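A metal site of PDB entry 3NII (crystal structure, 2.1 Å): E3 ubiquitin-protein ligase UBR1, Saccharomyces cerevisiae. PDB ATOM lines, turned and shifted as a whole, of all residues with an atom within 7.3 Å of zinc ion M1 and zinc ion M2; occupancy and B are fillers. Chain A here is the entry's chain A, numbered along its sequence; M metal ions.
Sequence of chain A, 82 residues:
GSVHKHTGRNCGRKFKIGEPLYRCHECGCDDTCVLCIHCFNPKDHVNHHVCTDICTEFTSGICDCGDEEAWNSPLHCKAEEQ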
ATOM      1  N   HIS A   4       1.751  -1.797  13.967  1.00  0.00           N
ATOM      2  CA  HIS A   4       2.698  -0.970  14.725  1.00  0.00           C
ATOM      3  C   HIS A   4       3.755  -1.794  15.457  1.00  0.00           C
ATOM      4  O   HIS A   4       4.556  -1.256  16.232  1.00  0.00           O
ATOM      5  CB  HIS A   4       1.948  -0.075  15.709  1.00  0.00           C
ATOM      6  CG  HIS A   4       0.519   0.166  15.349  1.00  0.00           C
ATOM      7  ND1 HIS A   4       0.138   1.079  14.388  1.00  0.00           N
ATOM      8  CD2 HIS A   4      -0.625  -0.383  15.819  1.00  0.00           C
ATOM      9  CE1 HIS A   4      -1.179   1.083  14.272  1.00  0.00           C
ATOM     10  NE2 HIS A   4      -1.673   0.203  15.135  1.00  0.00           N
ATOM     11  N   LYS A   5       3.762  -3.103  15.193  1.00  0.00           N
ATOM     12  CA  LYS A   5       4.774  -4.019  15.730  1.00  0.00           C
ATOM     13  C   LYS A   5       6.152  -3.615  15.250  1.00  0.00           C
ATOM     14  O   LYS A   5       6.321  -3.124  14.123  1.00  0.00           O
ATOM     15  CB  LYS A   5       4.482  -5.459  15.278  1.00  0.00           C
ATOM     16  CG  LYS A   5       3.146  -6.017  15.746  1.00  0.00           C
ATOM     17  CD  LYS A   5       2.892  -7.406  15.178  1.00  0.00           C
ATOM     18  CE  LYS A   5       1.539  -7.941  15.631  1.00  0.00           C
ATOM     19  NZ  LYS A   5       1.263  -9.300  15.087  1.00  0.00           N
ATOM     20  N   HIS A   6       7.153  -3.810  16.101  1.00  0.00           N
ATOM     21  CA  HIS A   6       8.542  -3.463  15.784  1.00  0.00           C
ATOM     22  C   HIS A   6       9.513  -4.454  16.430  1.00  0.00           C
ATOM     23  O   HIS A   6      10.574  -4.062  16.923  1.00  0.00           O
ATOM     24  CB  HIS A   6       8.843  -2.020  16.206  1.00  0.00           C
ATOM     25  CG  HIS A   6       8.703  -1.780  17.671  1.00  0.00           C
ATOM     26  ND1 HIS A   6       9.735  -1.968  18.566  1.00  0.00           N
ATOM     27  CD2 HIS A   6       7.636  -1.377  18.409  1.00  0.00           C
ATOM     28  CE1 HIS A   6       9.315  -1.679  19.775  1.00  0.00           C
ATOM     29  NE2 HIS A   6       8.054  -1.316  19.712  1.00  0.00           N
ATOM     30  N   THR A   7       9.139  -5.729  16.411  1.00  0.00           N
ATOM     31  CA  THR A   7       9.930  -6.816  17.000  1.00  0.00           C
ATOM     32  C   THR A   7      11.425  -6.681  16.708  1.00  0.00           C
ATOM     33  O   THR A   7      11.837  -6.540  15.562  1.00  0.00           O
ATOM     34  CB  THR A   7       9.433  -8.198  16.484  1.00  0.00           C
ATOM     35  OG1 THR A   7       7.997  -8.214  16.449  1.00  0.00           O
ATOM     36  CG2 THR A   7       9.938  -9.329  17.371  1.00  0.00           C
ATOM     37  N   ARG A   9      13.637  -4.337  17.603  1.00  0.00           N
ATOM     38  CA  ARG A   9      14.205  -2.983  17.562  1.00  0.00           C
ATOM     39  C   ARG A   9      13.330  -2.001  18.324  1.00  0.00           C
ATOM     40  O   ARG A   9      12.267  -2.370  18.836  1.00  0.00           O
ATOM     41  CB  ARG A   9      14.457  -2.513  16.112  1.00  0.00           C
ATOM     42  CG  ARG A   9      13.273  -2.700  15.155  1.00  0.00           C
ATOM     43  CD  ARG A   9      13.274  -1.667  14.037  1.00  0.00           C
ATOM     44  NE  ARG A   9      12.802  -0.366  14.512  1.00  0.00           N
ATOM     45  CZ  ARG A   9      12.447   0.639  13.723  1.00  0.00           C
ATOM     46  NH1 ARG A   9      12.502   0.519  12.403  1.00  0.00           N
ATOM     47  NH2 ARG A   9      12.033   1.778  14.261  1.00  0.00           N
ATOM     48  N   ASN A  10      13.788  -0.755  18.429  1.00  0.00           N
ATOM     49  CA  ASN A  10      13.026   0.288  19.104  1.00  0.00           C
ATOM     50  C   ASN A  10      11.811   0.712  18.262  1.00  0.00           C
ATOM     51  O   ASN A  10      11.797   0.525  17.036  1.00  0.00           O
ATOM     52  CB  ASN A  10      13.928   1.509  19.367  1.00  0.00           C
ATOM     53  CG  ASN A  10      14.295   2.254  18.102  1.00  0.00           C
ATOM     54  OD1 ASN A  10      14.916   1.693  17.193  1.00  0.00           O
ATOM     55  ND2 ASN A  10      13.929   3.527  18.024  1.00  0.00           N
ATOM     56  N   CYS A  11      10.796   1.269  18.921  1.00  0.00           N
ATOM     57  CA  CYS A  11       9.633   1.788  18.204  1.00  0.00           C
ATOM     58  C   CYS A  11      10.036   3.035  17.405  1.00  0.00           C
ATOM     59  O   CYS A  11      10.021   3.021  16.173  1.00  0.00           O
ATOM     60  CB  CYS A  11       8.477   2.084  19.162  1.00  0.00           C
ATOM     61  SG  CYS A  11       7.013   2.738  18.326  1.00  0.00           S
ATOM     62  N   GLY A  12      10.414   4.084  18.122  1.00  0.00           N
ATOM     63  CA  GLY A  12      10.854   5.328  17.482  1.00  0.00           C
ATOM     64  C   GLY A  12       9.754   6.124  16.799  1.00  0.00           C
ATOM     65  O   GLY A  12      10.034   7.111  16.119  1.00  0.00           O
ATOM     66  N   ARG A  13       8.494   5.700  16.971  1.00  0.00           N
ATOM     67  CA  ARG A  13       7.335   6.426  16.436  1.00  0.00           C
ATOM     68  C   ARG A  13       7.327   7.852  16.956  1.00  0.00           C
ATOM     69  O   ARG A  13       7.286   8.077  18.160  1.00  0.00           O
ATOM     70  CB  ARG A  13       6.027   5.717  16.809  1.00  0.00           C
ATOM     71  CG  ARG A  13       4.748   6.478  16.417  1.00  0.00           C
ATOM     72  CD  ARG A  13       3.505   5.684  16.780  1.00  0.00           C
ATOM     73  NE  ARG A  13       3.115   4.814  15.688  1.00  0.00           N
ATOM     74  CZ  ARG A  13       2.235   5.149  14.747  1.00  0.00           C
ATOM     75  NH1 ARG A  13       1.635   6.340  14.786  1.00  0.00           N
ATOM     76  NH2 ARG A  13       1.946   4.300  13.764  1.00  0.00           N
ATOM     77  N   PHE A  15       5.828  11.395  17.848  1.00  0.00           N
ATOM     78  CA  PHE A  15       4.544  11.922  18.286  1.00  0.00           C
ATOM     79  C   PHE A  15       4.127  13.157  17.495  1.00  0.00           C
ATOM     80  O   PHE A  15       4.964  13.970  17.110  1.00  0.00           O
ATOM     81  CB  PHE A  15       4.564  12.259  19.785  1.00  0.00           C
ATOM     82  CG  PHE A  15       4.735  11.061  20.674  1.00  0.00           C
ATOM     83  CD1 PHE A  15       3.628  10.280  21.032  1.00  0.00           C
ATOM     84  CD2 PHE A  15       5.984  10.712  21.162  1.00  0.00           C
ATOM     85  CE1 PHE A  15       3.789   9.170  21.855  1.00  0.00           C
ATOM     86  CE2 PHE A  15       6.153   9.597  21.987  1.00  0.00           C
ATOM     87  CZ  PHE A  15       5.067   8.825  22.335  1.00  0.00           C
ATOM     88  N   VAL A  34       9.312   7.766  27.201  1.00  0.00           N
ATOM     89  CA  VAL A  34       7.892   7.753  26.831  1.00  0.00           C
ATOM     90  C   VAL A  34       7.464   6.568  25.966  1.00  0.00           C
ATOM     91  O   VAL A  34       8.282   5.954  25.282  1.00  0.00           O
ATOM     92  CB  VAL A  34       7.465   9.060  26.088  1.00  0.00           C
ATOM     93  CG1 VAL A  34       7.546  10.265  27.010  1.00  0.00           C
ATOM     94  CG2 VAL A  34       8.314   9.299  24.857  1.00  0.00           C
ATOM     95  N   LEU A  35       6.166   6.272  25.991  1.00  0.00           N
ATOM     96  CA  LEU A  35       5.571   5.235  25.165  1.00  0.00           C
ATOM     97  C   LEU A  35       4.397   5.807  24.387  1.00  0.00           C
ATOM     98  O   LEU A  35       3.688   6.676  24.891  1.00  0.00           O
ATOM     99  CB  LEU A  35       5.084   4.065  26.023  1.00  0.00           C
ATOM    100  CG  LEU A  35       6.135   3.288  26.818  1.00  0.00           C
ATOM    101  CD1 LEU A  35       5.502   2.542  27.990  1.00  0.00           C
ATOM    102  CD2 LEU A  35       6.891   2.319  25.907  1.00  0.00           C
ATOM    103  N   CYS A  36       4.202   5.330  23.164  1.00  0.00           N
ATOM    104  CA  CYS A  36       3.031   5.689  22.368  1.00  0.00           C
ATOM    105  C   CYS A  36       1.846   4.804  22.743  1.00  0.00           C
ATOM    106  O   CYS A  36       2.014   3.806  23.448  1.00  0.00           O
ATOM    107  CB  CYS A  36       3.329   5.591  20.870  1.00  0.00           C
ATOM    108  SG  CYS A  36       3.437   3.909  20.207  1.00  0.00           S
ATOM    109  N   ILE A  37       0.665   5.153  22.233  1.00  0.00           N
ATOM    110  CA  ILE A  37      -0.569   4.422  22.537  1.00  0.00           C
ATOM    111  C   ILE A  37      -0.535   2.975  22.002  1.00  0.00           C
ATOM    112  O   ILE A  37      -1.110   2.074  22.604  1.00  0.00           O
ATOM    113  CB  ILE A  37      -1.858   5.197  22.070  1.00  0.00           C
ATOM    114  CG1 ILE A  37      -3.122   4.624  22.723  1.00  0.00           C
ATOM    115  CG2 ILE A  37      -1.942   5.248  20.524  1.00  0.00           C
ATOM    116  CD1 ILE A  37      -4.344   5.557  22.728  1.00  0.00           C
ATOM    117  N   HIS A  38       0.166   2.763  20.895  1.00  0.00           N
ATOM    118  CA  HIS A  38       0.258   1.431  20.298  1.00  0.00           C
ATOM    119  C   HIS A  38       1.191   0.502  21.083  1.00  0.00           C
ATOM    120  O   HIS A  38       1.083  -0.725  20.976  1.00  0.00           O
ATOM    121  CB  HIS A  38       0.712   1.532  18.838  1.00  0.00           C
ATOM    122  CG  HIS A  38      -0.078   2.515  18.031  1.00  0.00           C
ATOM    123  ND1 HIS A  38      -1.453   2.493  17.984  1.00  0.00           N
ATOM    124  CD2 HIS A  38       0.318   3.547  17.255  1.00  0.00           C
ATOM    125  CE1 HIS A  38      -1.878   3.475  17.210  1.00  0.00           C
ATOM    126  NE2 HIS A  38      -0.826   4.128  16.754  1.00  0.00           N
ATOM    127  N   CYS A  39       2.073   1.095  21.890  1.00  0.00           N
ATOM    128  CA  CYS A  39       3.096   0.345  22.617  1.00  0.00           C
ATOM    129  C   CYS A  39       2.768   0.167  24.103  1.00  0.00           C
ATOM    130  O   CYS A  39       2.997  -0.910  24.675  1.00  0.00           O
ATOM    131  CB  CYS A  39       4.462   1.028  22.458  1.00  0.00           C
ATOM    132  SG  CYS A  39       5.232   0.960  20.787  1.00  0.00           S
ATOM    133  N   PHE A  40       2.246   1.219  24.734  1.00  0.00           N
ATOM    134  CA  PHE A  40       1.906   1.182  26.166  1.00  0.00           C
ATOM    135  C   PHE A  40       0.968   0.017  26.502  1.00  0.00           C
ATOM    136  O   PHE A  40      -0.148  -0.079  25.967  1.00  0.00           O
ATOM    137  CB  PHE A  40       1.302   2.503  26.623  1.00  0.00           C
ATOM    138  CG  PHE A  40       0.911   2.530  28.091  1.00  0.00           C
ATOM    139  CD1 PHE A  40       1.863   2.800  29.068  1.00  0.00           C
ATOM    140  CD2 PHE A  40      -0.410   2.301  28.479  1.00  0.00           C
ATOM    141  CE1 PHE A  40       1.503   2.835  30.426  1.00  0.00           C
ATOM    142  CE2 PHE A  40      -0.775   2.326  29.828  1.00  0.00           C
ATOM    143  CZ  PHE A  40       0.186   2.589  30.798  1.00  0.00           C
ATOM    144  N   ILE A  62       9.886  10.954  20.424  1.00  0.00           N
ATOM    145  CA  ILE A  62       9.635   9.616  19.890  1.00  0.00           C
ATOM    146  C   ILE A  62       9.421   8.574  20.984  1.00  0.00           C
ATOM    147  O   ILE A  62       9.874   8.734  22.114  1.00  0.00           O
ATOM    148  CB  ILE A  62      10.785   9.138  18.939  1.00  0.00           C
ATOM    149  CG1 ILE A  62      12.120   9.103  19.693  1.00  0.00           C
ATOM    150  CG2 ILE A  62      10.878  10.035  17.710  1.00  0.00           C
ATOM    151  CD1 ILE A  62      13.104   8.082  19.153  1.00  0.00           C
ATOM    152  N   CYS A  63       8.733   7.501  20.622  1.00  0.00           N
ATOM    153  CA  CYS A  63       8.437   6.407  21.531  1.00  0.00           C
ATOM    154  C   CYS A  63       9.714   5.618  21.846  1.00  0.00           C
ATOM    155  O   CYS A  63      10.513   5.347  20.943  1.00  0.00           O
ATOM    156  CB  CYS A  63       7.385   5.492  20.907  1.00  0.00           C
ATOM    157  SG  CYS A  63       6.992   4.054  21.889  1.00  0.00           S
ATOM    158  N   ASP A  64       9.874   5.270  23.121  1.00  0.00           N
ATOM    159  CA  ASP A  64      11.068   4.577  23.605  1.00  0.00           C
ATOM    160  C   ASP A  64      10.888   3.076  23.786  1.00  0.00           C
ATOM    161  O   ASP A  64      11.791   2.395  24.264  1.00  0.00           O
ATOM    162  CB  ASP A  64      11.565   5.223  24.898  1.00  0.00           C
ATOM    163  CG  ASP A  64      11.948   6.676  24.717  1.00  0.00           C
ATOM    164  OD1 ASP A  64      12.747   6.949  23.811  1.00  0.00           O
ATOM    165  OD2 ASP A  64      11.421   7.540  25.447  1.00  0.00           O
ATOM    166  N   CYS A  65       9.714   2.563  23.411  1.00  0.00           N
ATOM    167  CA  CYS A  65       9.451   1.128  23.502  1.00  0.00           C
ATOM    168  C   CYS A  65      10.502   0.339  22.730  1.00  0.00           C
ATOM    169  O   CYS A  65      10.799   0.650  21.576  1.00  0.00           O
ATOM    170  CB  CYS A  65       8.066   0.795  22.972  1.00  0.00           C
ATOM    171  SG  CYS A  65       7.551  -0.913  23.268  1.00  0.00           S
ATOM    172  N   GLY A  66      11.068  -0.679  23.373  1.00  0.00           N
ATOM    173  CA  GLY A  66      12.103  -1.495  22.757  1.00  0.00           C
ATOM    174  C   GLY A  66      13.508  -0.955  22.910  1.00  0.00           C
ATOM    175  O   GLY A  66      14.479  -1.632  22.560  1.00  0.00           O
ATOM    176  N   HIS A  76       6.404  -5.189  27.660  1.00  0.00           N
ATOM    177  CA  HIS A  76       5.770  -6.095  26.707  1.00  0.00           C
ATOM    178  C   HIS A  76       4.858  -5.304  25.783  1.00  0.00           C
ATOM    179  O   HIS A  76       3.695  -5.045  26.114  1.00  0.00           O
ATOM    180  CB  HIS A  76       4.993  -7.188  27.437  1.00  0.00           C
ATOM    181  CG  HIS A  76       5.783  -7.895  28.496  1.00  0.00           C
ATOM    182  ND1 HIS A  76       5.794  -7.490  29.810  1.00  0.00           N
ATOM    183  CD2 HIS A  76       6.618  -8.961  28.415  1.00  0.00           C
ATOM    184  CE1 HIS A  76       6.591  -8.288  30.508  1.00  0.00           C
ATOM    185  NE2 HIS A  76       7.098  -9.195  29.680  1.00  0.00           N
ATOM    186  N   CYS A  77       5.408  -4.917  24.626  1.00  0.00           N
ATOM    187  CA  CYS A  77       4.741  -4.084  23.633  1.00  0.00           C
ATOM    188  C   CYS A  77       3.286  -4.507  23.404  1.00  0.00           C
ATOM    189  O   CYS A  77       3.008  -5.682  23.167  1.00  0.00           O
ATOM    190  CB  CYS A  77       5.512  -4.129  22.305  1.00  0.00           C
ATOM    191  SG  CYS A  77       5.231  -2.745  21.160  1.00  0.00           S
ATOM    192  N   LYS A  78       2.368  -3.541  23.492  1.00  0.00           N
ATOM    193  CA  LYS A  78       0.944  -3.802  23.242  1.00  0.00           C
ATOM    194  C   LYS A  78       0.663  -4.146  21.774  1.00  0.00           C
ATOM    195  O   LYS A  78      -0.213  -4.968  21.483  1.00  0.00           O
ATOM    196  CB  LYS A  78       0.065  -2.629  23.689  1.00  0.00           C
ATOM    197  CG  LYS A  78      -1.408  -3.009  23.889  1.00  0.00           C
ATOM    198  CD  LYS A  78      -2.306  -1.781  24.040  1.00  0.00           C
ATOM    199  CE  LYS A  78      -2.748  -1.222  22.688  1.00  0.00           C
ATOM    200  NZ  LYS A  78      -3.858  -2.020  22.080  1.00  0.00           N
ATOM    201  N   ALA A  79       1.409  -3.527  20.859  1.00  0.00           N
ATOM    202  CA  ALA A  79       1.303  -3.822  19.425  1.00  0.00           C
ATOM    203  C   ALA A  79       1.601  -5.294  19.129  1.00  0.00           C
ATOM    204  O   ALA A  79       1.046  -5.884  18.208  1.00  0.00           O
ATOM    205  CB  ALA A  79       2.214  -2.918  18.618  1.00  0.00           C
ATOM    206  N   GLU A  80       2.486  -5.876  19.946  1.00  0.00           N
ATOM    207  CA  GLU A  80       2.891  -7.277  19.835  1.00  0.00           C
ATOM    208  C   GLU A  80       1.773  -8.243  20.271  1.00  0.00           C
ATOM    209  O   GLU A  80       1.917  -9.467  20.162  1.00  0.00           O
ATOM    210  CB  GLU A  80       4.160  -7.506  20.663  1.00  0.00           C
ATOM    211  CG  GLU A  80       5.071  -8.631  20.171  1.00  0.00           C
ATOM    212  CD  GLU A  80       5.952  -8.226  18.990  1.00  0.00           C
ATOM    213  OE1 GLU A  80       5.994  -7.035  18.616  1.00  0.00           O
ATOM    214  OE2 GLU A  80       6.607  -9.134  18.434  1.00  0.00           O
HETATM  215 ZN    ZN M   1       5.662   3.000  20.306  1.00  0.00          ZN
HETATM  216 ZN    ZN M   2       6.269  -1.071  21.195  1.00  0.00          ZN
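The backbone NH of Arg 13 sits close to the side-chain sulfur of Cys 11, at 3.6 Å.
The backbone carbonyl oxygen (O) of Arg 13 is in hydrogen-bond range of the backbone NH (N) of Cys 63, at 2.9 Å.
O of Cys 11 sits at hydrogen-bond distance from NH2 of Arg 9 (3.0 Å).
The backbone NH (N) of Cys 11 lies close to a ring nitrogen (ND1) of His 6.
The backbone NH of Gly 12 is in hydrogen-bond range of the backbone carbonyl oxygen of Cys 63, at 3.1 Å.
The backbone NH (N) of Cys 11 lies within hydrogen-bond range of the backbone carbonyl oxygen (O) of Cys 65, at 2.7 Å.
O of Arg 9 lies within hydrogen-bond range of ND1 of His 6, 2.6 Å away.
N of Cys 65 sits close to SG of Cys 63 (3.5 Å).
Four residues have an atom within 4 Å of zinc ion M1: Cys 11, Cys 36, Cys 39 and Cys 63.
Along chain A the residues within 4 Å of zinc ion M1 span positions 11 to 63.
Within 4 Å of zinc ion M2: His 6, Cys 39, Cys 65 and Cys 77.
Zinc ion M1 is bound by the side-chain sulfur (SG) of Cys 39, the side-chain sulfur (SG) of Cys 63, the side-chain sulfur (SG) of Cys 36 and the side-chain sulfur (SG) of Cys 11.
Zinc ion M1 has four donor atoms within binding distance.
Zinc ion M2 is bound by the side-chain sulfur of Cys 77 (2.0 Å), the side-chain sulfur of Cys 39 (2.3 Å), a ring nitrogen (NE2) of His 6 (2.3 Å) and the side-chain sulfur of Cys 65 (2.4 Å).
Zinc ion M2 has four donor atoms within binding distance.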
